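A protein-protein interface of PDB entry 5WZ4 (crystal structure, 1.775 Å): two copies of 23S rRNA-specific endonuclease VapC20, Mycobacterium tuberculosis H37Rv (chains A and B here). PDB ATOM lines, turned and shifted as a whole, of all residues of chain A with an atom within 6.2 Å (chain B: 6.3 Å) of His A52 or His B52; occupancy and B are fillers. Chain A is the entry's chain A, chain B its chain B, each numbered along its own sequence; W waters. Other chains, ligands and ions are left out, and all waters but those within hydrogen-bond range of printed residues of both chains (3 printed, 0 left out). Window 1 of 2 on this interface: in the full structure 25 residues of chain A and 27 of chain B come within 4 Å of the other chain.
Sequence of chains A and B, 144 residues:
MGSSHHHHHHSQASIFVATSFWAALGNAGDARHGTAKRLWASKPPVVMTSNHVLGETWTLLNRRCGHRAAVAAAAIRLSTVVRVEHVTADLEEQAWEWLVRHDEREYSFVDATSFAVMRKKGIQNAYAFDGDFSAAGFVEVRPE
Hydrophobic or aromatic side chains of chain B within 4 Å of the printed part of chain A: His B52, His B86 and Phe B109. Of the 17 printed residues of chain A, 7 touch a printed residue of chain B. Printed residues of chain A that touch a printed residue of chain B: Asn A51, His A52, Gly A55, His A86, Val A87, Glu A92 and Phe A109. Hydrophobic or aromatic side chains of chain A that line the printed part of chain B: His A52, His A86 and Phe A109. Among the printed residues, 9 pairs touch across the chains. Among the printed residues, no Asp or Glu carboxylate lies within 4 Å of a Lys or Arg side-chain nitrogen of the other chain.
Thr A57 touches none of the printed residues of chain B. Of the printed residues of chain B, His A86 touches His B86, Val B87 and Glu B92. Printed residues of chain B within 4 Å of Phe A109: Gly B55. Of the printed residues of chain A, Asn B51 touches Glu A92 (2.8 Å). Of the printed residues of chain A, His B52 touches His A52. Of the printed residues of chain A, Val B87 touches His A86. Of the printed residues of chain A, Glu B92 touches Asn A51 and His A86. The nearest printed residue of chain B that does not touch His A52 is Asn B51 (4.2 Å). The nearest printed residue of chain A that does not touch Asn B51 is His A52 (4.2 Å).
The side-chain amide nitrogen (ND2) of Asn A51 lies within hydrogen-bond range of the side-chain carboxylate (OE2) of Glu B92 (2.7 Å). NE2 of His A86 sits at hydrogen-bond distance from NE2 of His B86 (2.9 Å). The side-chain carboxylate of Glu A92 lies within hydrogen-bond range of the side-chain amide nitrogen of Asn B51.
Asn A51 touches Glu B92, and with the chains exchanged Glu A92 touches Asn B51. Gly A55 touches Phe B109, and with the chains exchanged Phe A109 touches Gly B55. His A86 touches its own counterpart, His B86. His A86 touches Val B87, and with the chains exchanged Val A87 touches His B86. 17 positions are printed for both chains. Of the 9 pairs that touch across the chains among the printed residues, 8 have their exchanged pair printed and touching as well.
Among the printed residues, merely in contact across the chains: Phe A109 with Gly B55, Gly A55 with Phe B109, Val A87 with His B86, His A86 with Val B87, His A52 with His B52 and His A86 with Glu B92.
Water W1 lies within hydrogen-bond range of OE1 of Glu B92 (2.6 Å) and ND1 of His A86 (2.7 Å). Water W3 lies within hydrogen-bond range of ND1 of His B86 (2.6 Å) and OE1 of Glu A92 (2.6 Å). Water W2 lies within hydrogen-bond range of the backbone carbonyl oxygen of Asn A51 and the side-chain carboxylate of Glu B92.
O of Glu A85 lies within hydrogen-bond range of N of Asn A51. N of Val A87 sits at hydrogen-bond distance from OD1 of Asn A51, at 3.0 Å. A ring nitrogen (NE2) of His A52 sits at hydrogen-bond distance from the side-chain carboxylate (OE2) of Glu A92 (2.6 Å). N of His B52 lies close to OG of Ser B50, at 3.3 Å. A ring nitrogen (NE2) of His B52 is in hydrogen-bond range of the side-chain carboxylate (OE2) of Glu B92 (3.0 Å). A ring nitrogen (ND1) of His B52 lies within hydrogen-bond range of the side-chain hydroxyl of Thr B113, 3.3 Å away.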
ATOM      1  N   THR A  19     -20.246  -8.255  31.603  1.00  0.00           N
ATOM      2  CA  THR A  19     -20.599  -8.776  30.286  1.00  0.00           C
ATOM      3  C   THR A  19     -22.012  -9.343  30.246  1.00  0.00           C
ATOM      4  O   THR A  19     -22.727  -9.164  29.262  1.00  0.00           O
ATOM      5  CB  THR A  19     -19.616  -9.867  29.838  1.00  0.00           C
ATOM      6  OG1 THR A  19     -18.299  -9.311  29.753  1.00  0.00           O
ATOM      7  CG2 THR A  19     -20.010 -10.431  28.483  1.00  0.00           C
ATOM      8  N   SER A  50     -14.991  -2.286  32.185  1.00  0.00           N
ATOM      9  CA  SER A  50     -13.560  -2.453  31.960  1.00  0.00           C
ATOM     10  C   SER A  50     -13.249  -2.822  30.522  1.00  0.00           C
ATOM     11  O   SER A  50     -14.135  -3.210  29.765  1.00  0.00           O
ATOM     12  CB  SER A  50     -12.989  -3.524  32.886  1.00  0.00           C
ATOM     13  OG  SER A  50     -13.356  -4.817  32.439  1.00  0.00           O
ATOM     14  N   ASN A  51     -11.976  -2.707  30.159  1.00  0.00           N
ATOM     15  CA  ASN A  51     -11.526  -3.122  28.842  1.00  0.00           C
ATOM     16  C   ASN A  51     -11.733  -4.620  28.656  1.00  0.00           C
ATOM     17  O   ASN A  51     -12.115  -5.066  27.574  1.00  0.00           O
ATOM     18  CB  ASN A  51     -10.054  -2.749  28.620  1.00  0.00           C
ATOM     19  CG  ASN A  51      -9.119  -3.382  29.641  1.00  0.00           C
ATOM     20  OD1 ASN A  51      -9.407  -3.415  30.837  1.00  0.00           O
ATOM     21  ND2 ASN A  51      -7.988  -3.892  29.164  1.00  0.00           N
ATOM     22  N   HIS A  52     -11.502  -5.392  29.717  1.00  0.00           N
ATOM     23  CA  HIS A  52     -11.708  -6.841  29.665  1.00  0.00           C
ATOM     24  C   HIS A  52     -13.168  -7.191  29.401  1.00  0.00           C
ATOM     25  O   HIS A  52     -13.470  -8.116  28.647  1.00  0.00           O
ATOM     26  CB  HIS A  52     -11.263  -7.510  30.968  1.00  0.00           C
ATOM     27  CG  HIS A  52      -9.779  -7.556  31.153  1.00  0.00           C
ATOM     28  ND1 HIS A  52      -8.914  -7.942  30.152  1.00  0.00           N
ATOM     29  CD2 HIS A  52      -9.008  -7.295  32.235  1.00  0.00           C
ATOM     30  CE1 HIS A  52      -7.673  -7.897  30.603  1.00  0.00           C
ATOM     31  NE2 HIS A  52      -7.702  -7.508  31.865  1.00  0.00           N
ATOM     32  N   VAL A  53     -14.069  -6.455  30.038  1.00  0.00           N
ATOM     33  CA  VAL A  53     -15.493  -6.723  29.907  1.00  0.00           C
ATOM     34  C   VAL A  53     -15.986  -6.426  28.494  1.00  0.00           C
ATOM     35  O   VAL A  53     -16.718  -7.224  27.907  1.00  0.00           O
ATOM     36  CB  VAL A  53     -16.314  -5.908  30.924  1.00  0.00           C
ATOM     37  CG1 VAL A  53     -17.785  -5.920  30.550  1.00  0.00           C
ATOM     38  CG2 VAL A  53     -16.112  -6.464  32.329  1.00  0.00           C
ATOM     39  N   LEU A  54     -15.581  -5.283  27.948  1.00  0.00           N
ATOM     40  CA  LEU A  54     -15.981  -4.901  26.597  1.00  0.00           C
ATOM     41  C   LEU A  54     -15.481  -5.925  25.589  1.00  0.00           C
ATOM     42  O   LEU A  54     -16.206  -6.315  24.676  1.00  0.00           O
ATOM     43  CB  LEU A  54     -15.458  -3.508  26.240  1.00  0.00           C
ATOM     44  CG  LEU A  54     -16.117  -2.321  26.942  1.00  0.00           C
ATOM     45  CD1 LEU A  54     -15.692  -1.014  26.279  1.00  0.00           C
ATOM     46  CD2 LEU A  54     -17.632  -2.463  26.937  1.00  0.00           C
ATOM     47  N   GLY A  55     -14.242  -6.369  25.771  1.00  0.00           N
ATOM     48  CA  GLY A  55     -13.678  -7.391  24.914  1.00  0.00           C
ATOM     49  C   GLY A  55     -14.479  -8.677  24.977  1.00  0.00           C
ATOM     50  O   GLY A  55     -14.797  -9.275  23.947  1.00  0.00           O
ATOM     51  N   GLU A  56     -14.813  -9.094  26.195  1.00  0.00           N
ATOM     52  CA  GLU A  56     -15.605 -10.298  26.407  1.00  0.00           C
ATOM     53  C   GLU A  56     -16.998 -10.135  25.809  1.00  0.00           C
ATOM     54  O   GLU A  56     -17.556 -11.073  25.240  1.00  0.00           O
ATOM     55  CB  GLU A  56     -15.697 -10.617  27.903  1.00  0.00           C
ATOM     56  CG  GLU A  56     -16.442 -11.900  28.233  1.00  0.00           C
ATOM     57  CD  GLU A  56     -16.675 -12.065  29.724  1.00  0.00           C
ATOM     58  OE1 GLU A  56     -16.768 -11.039  30.424  1.00  0.00           O
ATOM     59  OE2 GLU A  56     -16.770 -13.215  30.200  1.00  0.00           O
ATOM     60  N   THR A  57     -17.549  -8.933  25.939  1.00  0.00           N
ATOM     61  CA  THR A  57     -18.866  -8.624  25.396  1.00  0.00           C
ATOM     62  C   THR A  57     -18.865  -8.696  23.874  1.00  0.00           C
ATOM     63  O   THR A  57     -19.782  -9.261  23.279  1.00  0.00           O
ATOM     64  CB  THR A  57     -19.340  -7.232  25.846  1.00  0.00           C
ATOM     65  OG1 THR A  57     -19.536  -7.238  27.264  1.00  0.00           O
ATOM     66  CG2 THR A  57     -20.648  -6.865  25.167  1.00  0.00           C
ATOM     67  N   GLU A  85     -12.474   1.512  32.500  1.00  0.00           N
ATOM     68  CA  GLU A  85     -11.188   1.302  33.162  1.00  0.00           C
ATOM     69  C   GLU A  85     -10.297   0.361  32.370  1.00  0.00           C
ATOM     70  O   GLU A  85     -10.710  -0.745  32.033  1.00  0.00           O
ATOM     71  CB  GLU A  85     -11.376   0.718  34.566  1.00  0.00           C
ATOM     72  CG  GLU A  85     -11.686   1.717  35.657  1.00  0.00           C
ATOM     73  CD  GLU A  85     -10.769   2.922  35.641  1.00  0.00           C
ATOM     74  OE1 GLU A  85      -9.541   2.737  35.780  1.00  0.00           O
ATOM     75  OE2 GLU A  85     -11.280   4.054  35.503  1.00  0.00           O
ATOM     76  N   HIS A  86      -9.074   0.788  32.082  1.00  0.00           N
ATOM     77  CA  HIS A  86      -8.072  -0.148  31.597  1.00  0.00           C
ATOM     78  C   HIS A  86      -7.470  -0.857  32.798  1.00  0.00           C
ATOM     79  O   HIS A  86      -6.788  -0.235  33.614  1.00  0.00           O
ATOM     80  CB  HIS A  86      -6.977   0.552  30.793  1.00  0.00           C
ATOM     81  CG  HIS A  86      -5.913  -0.378  30.301  1.00  0.00           C
ATOM     82  ND1 HIS A  86      -5.995  -1.027  29.087  1.00  0.00           N
ATOM     83  CD2 HIS A  86      -4.753  -0.789  30.868  1.00  0.00           C
ATOM     84  CE1 HIS A  86      -4.927  -1.786  28.923  1.00  0.00           C
ATOM     85  NE2 HIS A  86      -4.156  -1.658  29.988  1.00  0.00           N
ATOM     86  N   VAL A  87      -7.733  -2.152  32.920  1.00  0.00           N
ATOM     87  CA  VAL A  87      -7.210  -2.907  34.051  1.00  0.00           C
ATOM     88  C   VAL A  87      -5.687  -2.932  34.001  1.00  0.00           C
ATOM     89  O   VAL A  87      -5.097  -3.450  33.055  1.00  0.00           O
ATOM     90  CB  VAL A  87      -7.755  -4.343  34.080  1.00  0.00           C
ATOM     91  CG1 VAL A  87      -7.304  -5.041  35.349  1.00  0.00           C
ATOM     92  CG2 VAL A  87      -9.276  -4.332  33.995  1.00  0.00           C
ATOM     93  N   GLU A  92      -4.450  -6.664  37.636  1.00  0.00           N
ATOM     94  CA  GLU A  92      -4.506  -8.023  37.111  1.00  0.00           C
ATOM     95  C   GLU A  92      -3.786  -9.004  38.029  1.00  0.00           C
ATOM     96  O   GLU A  92      -4.243 -10.127  38.223  1.00  0.00           O
ATOM     97  CB  GLU A  92      -3.911  -8.087  35.707  1.00  0.00           C
ATOM     98  CG  GLU A  92      -4.794  -7.448  34.662  1.00  0.00           C
ATOM     99  CD  GLU A  92      -4.376  -7.787  33.256  1.00  0.00           C
ATOM    100  OE1 GLU A  92      -3.321  -8.430  33.086  1.00  0.00           O
ATOM    101  OE2 GLU A  92      -5.113  -7.417  32.321  1.00  0.00           O
ATOM    102  N   PHE A 109     -11.659 -15.175  34.562  1.00  0.00           N
ATOM    103  CA  PHE A 109     -10.641 -14.137  34.689  1.00  0.00           C
ATOM    104  C   PHE A 109     -11.256 -12.742  34.641  1.00  0.00           C
ATOM    105  O   PHE A 109     -10.899 -11.871  35.430  1.00  0.00           O
ATOM    106  CB  PHE A 109      -9.589 -14.280  33.588  1.00  0.00           C
ATOM    107  CG  PHE A 109      -8.587 -13.160  33.554  1.00  0.00           C
ATOM    108  CD1 PHE A 109      -7.558 -13.106  34.478  1.00  0.00           C
ATOM    109  CD2 PHE A 109      -8.670 -12.170  32.591  1.00  0.00           C
ATOM    110  CE1 PHE A 109      -6.633 -12.079  34.445  1.00  0.00           C
ATOM    111  CE2 PHE A 109      -7.746 -11.141  32.552  1.00  0.00           C
ATOM    112  CZ  PHE A 109      -6.727 -11.097  33.481  1.00  0.00           C
ATOM    113  N   VAL A 110     -12.185 -12.533  33.716  1.00  0.00           N
ATOM    114  CA  VAL A 110     -12.813 -11.225  33.576  1.00  0.00           C
ATOM    115  C   VAL A 110     -13.590 -10.870  34.846  1.00  0.00           C
ATOM    116  O   VAL A 110     -13.591  -9.719  35.279  1.00  0.00           O
ATOM    117  CB  VAL A 110     -13.742 -11.169  32.345  1.00  0.00           C
ATOM    118  CG1 VAL A 110     -14.496  -9.852  32.306  1.00  0.00           C
ATOM    119  CG2 VAL A 110     -12.928 -11.346  31.064  1.00  0.00           C
ATOM    120  N   THR A 113     -11.069  -9.702  37.468  1.00  0.00           N
ATOM    121  CA  THR A 113     -10.577  -8.357  37.196  1.00  0.00           C
ATOM    122  C   THR A 113     -11.690  -7.344  37.457  1.00  0.00           C
ATOM    123  O   THR A 113     -11.427  -6.224  37.886  1.00  0.00           O
ATOM    124  CB  THR A 113     -10.052  -8.197  35.753  1.00  0.00           C
ATOM    125  OG1 THR A 113     -11.099  -8.463  34.812  1.00  0.00           O
ATOM    126  CG2 THR A 113      -8.885  -9.143  35.500  1.00  0.00           C
ATOM    127  N   SER A 114     -12.933  -7.751  37.211  1.00  0.00           N
ATOM    128  CA  SER A 114     -14.084  -6.891  37.484  1.00  0.00           C
ATOM    129  C   SER A 114     -14.228  -6.622  38.982  1.00  0.00           C
ATOM    130  O   SER A 114     -14.476  -5.489  39.397  1.00  0.00           O
ATOM    131  CB  SER A 114     -15.366  -7.516  36.932  1.00  0.00           C
ATOM    132  OG  SER A 114     -15.321  -7.593  35.518  1.00  0.00           O
ATOM    133  N   THR B  19      -4.463 -18.783  22.920  1.00  0.00           N
ATOM    134  CA  THR B  19      -5.274 -19.520  23.886  1.00  0.00           C
ATOM    135  C   THR B  19      -5.525 -20.961  23.452  1.00  0.00           C
ATOM    136  O   THR B  19      -5.470 -21.882  24.266  1.00  0.00           O
ATOM    137  CB  THR B  19      -6.636 -18.836  24.107  1.00  0.00           C
ATOM    138  OG1 THR B  19      -6.438 -17.451  24.412  1.00  0.00           O
ATOM    139  CG2 THR B  19      -7.392 -19.501  25.240  1.00  0.00           C
ATOM    140  N   SER B  50       0.242 -13.235  25.888  1.00  0.00           N
ATOM    141  CA  SER B  50      -0.275 -11.978  26.424  1.00  0.00           C
ATOM    142  C   SER B  50      -1.123 -12.188  27.670  1.00  0.00           C
ATOM    143  O   SER B  50      -1.540 -13.308  27.968  1.00  0.00           O
ATOM    144  CB  SER B  50      -1.100 -11.243  25.373  1.00  0.00           C
ATOM    145  OG  SER B  50      -2.411 -11.773  25.316  1.00  0.00           O
ATOM    146  N   ASN B  51      -1.384 -11.100  28.388  1.00  0.00           N
ATOM    147  CA  ASN B  51      -2.236 -11.162  29.567  1.00  0.00           C
ATOM    148  C   ASN B  51      -3.650 -11.593  29.193  1.00  0.00           C
ATOM    149  O   ASN B  51      -4.277 -12.372  29.915  1.00  0.00           O
ATOM    150  CB  ASN B  51      -2.258  -9.813  30.298  1.00  0.00           C
ATOM    151  CG  ASN B  51      -2.746  -8.668  29.424  1.00  0.00           C
ATOM    152  OD1 ASN B  51      -2.432  -8.590  28.235  1.00  0.00           O
ATOM    153  ND2 ASN B  51      -3.522  -7.770  30.018  1.00  0.00           N
ATOM    154  N   HIS B  52      -4.142 -11.099  28.059  1.00  0.00           N
ATOM    155  CA  HIS B  52      -5.469 -11.463  27.567  1.00  0.00           C
ATOM    156  C   HIS B  52      -5.568 -12.958  27.301  1.00  0.00           C
ATOM    157  O   HIS B  52      -6.565 -13.600  27.642  1.00  0.00           O
ATOM    158  CB  HIS B  52      -5.799 -10.695  26.287  1.00  0.00           C
ATOM    159  CG  HIS B  52      -6.004  -9.228  26.497  1.00  0.00           C
ATOM    160  ND1 HIS B  52      -6.662  -8.435  25.583  1.00  0.00           N
ATOM    161  CD2 HIS B  52      -5.638  -8.409  27.512  1.00  0.00           C
ATOM    162  CE1 HIS B  52      -6.694  -7.191  26.026  1.00  0.00           C
ATOM    163  NE2 HIS B  52      -6.081  -7.148  27.195  1.00  0.00           N
ATOM    164  N   VAL B  53      -4.532 -13.502  26.675  1.00  0.00           N
ATOM    165  CA  VAL B  53      -4.500 -14.919  26.346  1.00  0.00           C
ATOM    166  C   VAL B  53      -4.487 -15.773  27.610  1.00  0.00           C
ATOM    167  O   VAL B  53      -5.224 -16.755  27.710  1.00  0.00           O
ATOM    168  CB  VAL B  53      -3.276 -15.263  25.471  1.00  0.00           C
ATOM    169  CG1 VAL B  53      -3.051 -16.765  25.430  1.00  0.00           C
ATOM    170  CG2 VAL B  53      -3.455 -14.704  24.065  1.00  0.00           C
ATOM    171  N   LEU B  54      -3.656 -15.398  28.579  1.00  0.00           N
ATOM    172  CA  LEU B  54      -3.566 -16.156  29.823  1.00  0.00           C
ATOM    173  C   LEU B  54      -4.886 -16.103  30.579  1.00  0.00           C
ATOM    174  O   LEU B  54      -5.313 -17.095  31.161  1.00  0.00           O
ATOM    175  CB  LEU B  54      -2.427 -15.634  30.699  1.00  0.00           C
ATOM    176  CG  LEU B  54      -1.017 -15.982  30.211  1.00  0.00           C
ATOM    177  CD1 LEU B  54       0.017 -15.673  31.283  1.00  0.00           C
ATOM    178  CD2 LEU B  54      -0.938 -17.445  29.787  1.00  0.00           C
ATOM    179  N   GLY B  55      -5.535 -14.943  30.554  1.00  0.00           N
ATOM    180  CA  GLY B  55      -6.842 -14.796  31.168  1.00  0.00           C
ATOM    181  C   GLY B  55      -7.888 -15.700  30.542  1.00  0.00           C
ATOM    182  O   GLY B  55      -8.661 -16.354  31.245  1.00  0.00           O
ATOM    183  N   GLU B  56      -7.913 -15.734  29.212  1.00  0.00           N
ATOM    184  CA  GLU B  56      -8.849 -16.574  28.476  1.00  0.00           C
ATOM    185  C   GLU B  56      -8.568 -18.051  28.738  1.00  0.00           C
ATOM    186  O   GLU B  56      -9.488 -18.862  28.866  1.00  0.00           O
ATOM    187  CB  GLU B  56      -8.767 -16.275  26.979  1.00  0.00           C
ATOM    188  CG  GLU B  56      -9.829 -16.971  26.139  1.00  0.00           C
ATOM    189  CD  GLU B  56      -9.726 -16.621  24.664  1.00  0.00           C
ATOM    190  OE1 GLU B  56      -8.603 -16.389  24.177  1.00  0.00           O
ATOM    191  OE2 GLU B  56     -10.770 -16.583  23.982  1.00  0.00           O
ATOM    192  N   THR B  57      -7.287 -18.386  28.818  1.00  0.00           N
ATOM    193  CA  THR B  57      -6.858 -19.756  29.075  1.00  0.00           C
ATOM    194  C   THR B  57      -7.286 -20.216  30.464  1.00  0.00           C
ATOM    195  O   THR B  57      -7.748 -21.347  30.632  1.00  0.00           O
ATOM    196  CB  THR B  57      -5.336 -19.890  28.929  1.00  0.00           C
ATOM    197  OG1 THR B  57      -4.956 -19.505  27.602  1.00  0.00           O
ATOM    198  CG2 THR B  57      -4.892 -21.329  29.186  1.00  0.00           C
ATOM    199  N   GLU B  85       3.229 -10.415  27.523  1.00  0.00           N
ATOM    200  CA  GLU B  85       3.005  -9.022  27.153  1.00  0.00           C
ATOM    201  C   GLU B  85       1.693  -8.487  27.721  1.00  0.00           C
ATOM    202  O   GLU B  85       0.640  -9.090  27.525  1.00  0.00           O
ATOM    203  CB  GLU B  85       3.004  -8.881  25.630  1.00  0.00           C
ATOM    204  CG  GLU B  85       3.259  -7.472  25.125  1.00  0.00           C
ATOM    205  CD  GLU B  85       4.711  -7.057  25.262  1.00  0.00           C
ATOM    206  OE1 GLU B  85       4.976  -5.840  25.303  1.00  0.00           O
ATOM    207  OE2 GLU B  85       5.587  -7.947  25.327  1.00  0.00           O
ATOM    208  N   HIS B  86       1.756  -7.362  28.430  1.00  0.00           N
ATOM    209  CA  HIS B  86       0.539  -6.666  28.828  1.00  0.00           C
ATOM    210  C   HIS B  86       0.062  -5.827  27.649  1.00  0.00           C
ATOM    211  O   HIS B  86       0.741  -4.887  27.230  1.00  0.00           O
ATOM    212  CB  HIS B  86       0.767  -5.782  30.059  1.00  0.00           C
ATOM    213  CG  HIS B  86      -0.452  -5.025  30.496  1.00  0.00           C
ATOM    214  ND1 HIS B  86      -1.185  -5.372  31.611  1.00  0.00           N
ATOM    215  CD2 HIS B  86      -1.066  -3.939  29.968  1.00  0.00           C
ATOM    216  CE1 HIS B  86      -2.197  -4.533  31.750  1.00  0.00           C
ATOM    217  NE2 HIS B  86      -2.149  -3.656  30.766  1.00  0.00           N
ATOM    218  N   VAL B  87      -1.095  -6.181  27.103  1.00  0.00           N
ATOM    219  CA  VAL B  87      -1.637  -5.460  25.961  1.00  0.00           C
ATOM    220  C   VAL B  87      -1.999  -4.035  26.361  1.00  0.00           C
ATOM    221  O   VAL B  87      -2.843  -3.812  27.228  1.00  0.00           O
ATOM    222  CB  VAL B  87      -2.870  -6.170  25.380  1.00  0.00           C
ATOM    223  CG1 VAL B  87      -3.397  -5.413  24.172  1.00  0.00           C
ATOM    224  CG2 VAL B  87      -2.515  -7.602  25.003  1.00  0.00           C
ATOM    225  N   GLU B  92      -5.008  -2.342  22.068  1.00  0.00           N
ATOM    226  CA  GLU B  92      -6.423  -2.689  22.100  1.00  0.00           C
ATOM    227  C   GLU B  92      -7.206  -1.836  21.106  1.00  0.00           C
ATOM    228  O   GLU B  92      -8.089  -2.337  20.409  1.00  0.00           O
ATOM    229  CB  GLU B  92      -6.993  -2.524  23.510  1.00  0.00           C
ATOM    230  CG  GLU B  92      -6.556  -3.622  24.467  1.00  0.00           C
ATOM    231  CD  GLU B  92      -7.201  -3.502  25.833  1.00  0.00           C
ATOM    232  OE1 GLU B  92      -8.087  -2.637  25.999  1.00  0.00           O
ATOM    233  OE2 GLU B  92      -6.823  -4.274  26.735  1.00  0.00           O
ATOM    234  N   PHE B 109     -12.157 -11.014  20.540  1.00  0.00           N
ATOM    235  CA  PHE B 109     -11.374  -9.863  20.964  1.00  0.00           C
ATOM    236  C   PHE B 109      -9.951 -10.265  21.349  1.00  0.00           C
ATOM    237  O   PHE B 109      -8.990  -9.597  20.970  1.00  0.00           O
ATOM    238  CB  PHE B 109     -12.055  -9.157  22.134  1.00  0.00           C
ATOM    239  CG  PHE B 109     -11.237  -8.048  22.731  1.00  0.00           C
ATOM    240  CD1 PHE B 109     -11.187  -6.803  22.130  1.00  0.00           C
ATOM    241  CD2 PHE B 109     -10.520  -8.254  23.900  1.00  0.00           C
ATOM    242  CE1 PHE B 109     -10.434  -5.783  22.681  1.00  0.00           C
ATOM    243  CE2 PHE B 109      -9.771  -7.241  24.457  1.00  0.00           C
ATOM    244  CZ  PHE B 109      -9.728  -6.002  23.847  1.00  0.00           C
ATOM    245  N   VAL B 110      -9.817 -11.352  22.106  1.00  0.00           N
ATOM    246  CA  VAL B 110      -8.497 -11.814  22.532  1.00  0.00           C
ATOM    247  C   VAL B 110      -7.614 -12.136  21.328  1.00  0.00           C
ATOM    248  O   VAL B 110      -6.442 -11.766  21.293  1.00  0.00           O
ATOM    249  CB  VAL B 110      -8.587 -13.054  23.446  1.00  0.00           C
ATOM    250  CG1 VAL B 110      -7.191 -13.612  23.729  1.00  0.00           C
ATOM    251  CG2 VAL B 110      -9.296 -12.704  24.746  1.00  0.00           C
ATOM    252  N   THR B 113      -6.456  -8.828  19.749  1.00  0.00           N
ATOM    253  CA  THR B 113      -5.347  -8.221  20.480  1.00  0.00           C
ATOM    254  C   THR B 113      -4.080  -9.037  20.273  1.00  0.00           C
ATOM    255  O   THR B 113      -2.979  -8.490  20.254  1.00  0.00           O
ATOM    256  CB  THR B 113      -5.640  -8.101  21.989  1.00  0.00           C
ATOM    257  OG1 THR B 113      -5.821  -9.401  22.564  1.00  0.00           O
ATOM    258  CG2 THR B 113      -6.887  -7.273  22.215  1.00  0.00           C
ATOM    259  N   SER B 114      -4.242 -10.348  20.118  1.00  0.00           N
ATOM    260  CA  SER B 114      -3.109 -11.216  19.825  1.00  0.00           C
ATOM    261  C   SER B 114      -2.494 -10.847  18.476  1.00  0.00           C
ATOM    262  O   SER B 114      -1.272 -10.759  18.350  1.00  0.00           O
ATOM    263  CB  SER B 114      -3.540 -12.684  19.836  1.00  0.00           C
ATOM    264  OG  SER B 114      -3.914 -13.086  21.142  1.00  0.00           O
HETATM  265  O   HOH W   1      -7.596  -0.305  27.048  1.00  0.00           O
HETATM  266  O   HOH W   2     -11.390  -3.121  25.573  1.00  0.00           O
HETATM  267  O   HOH W   3      -0.861  -7.467  33.156  1.00  0.00           O
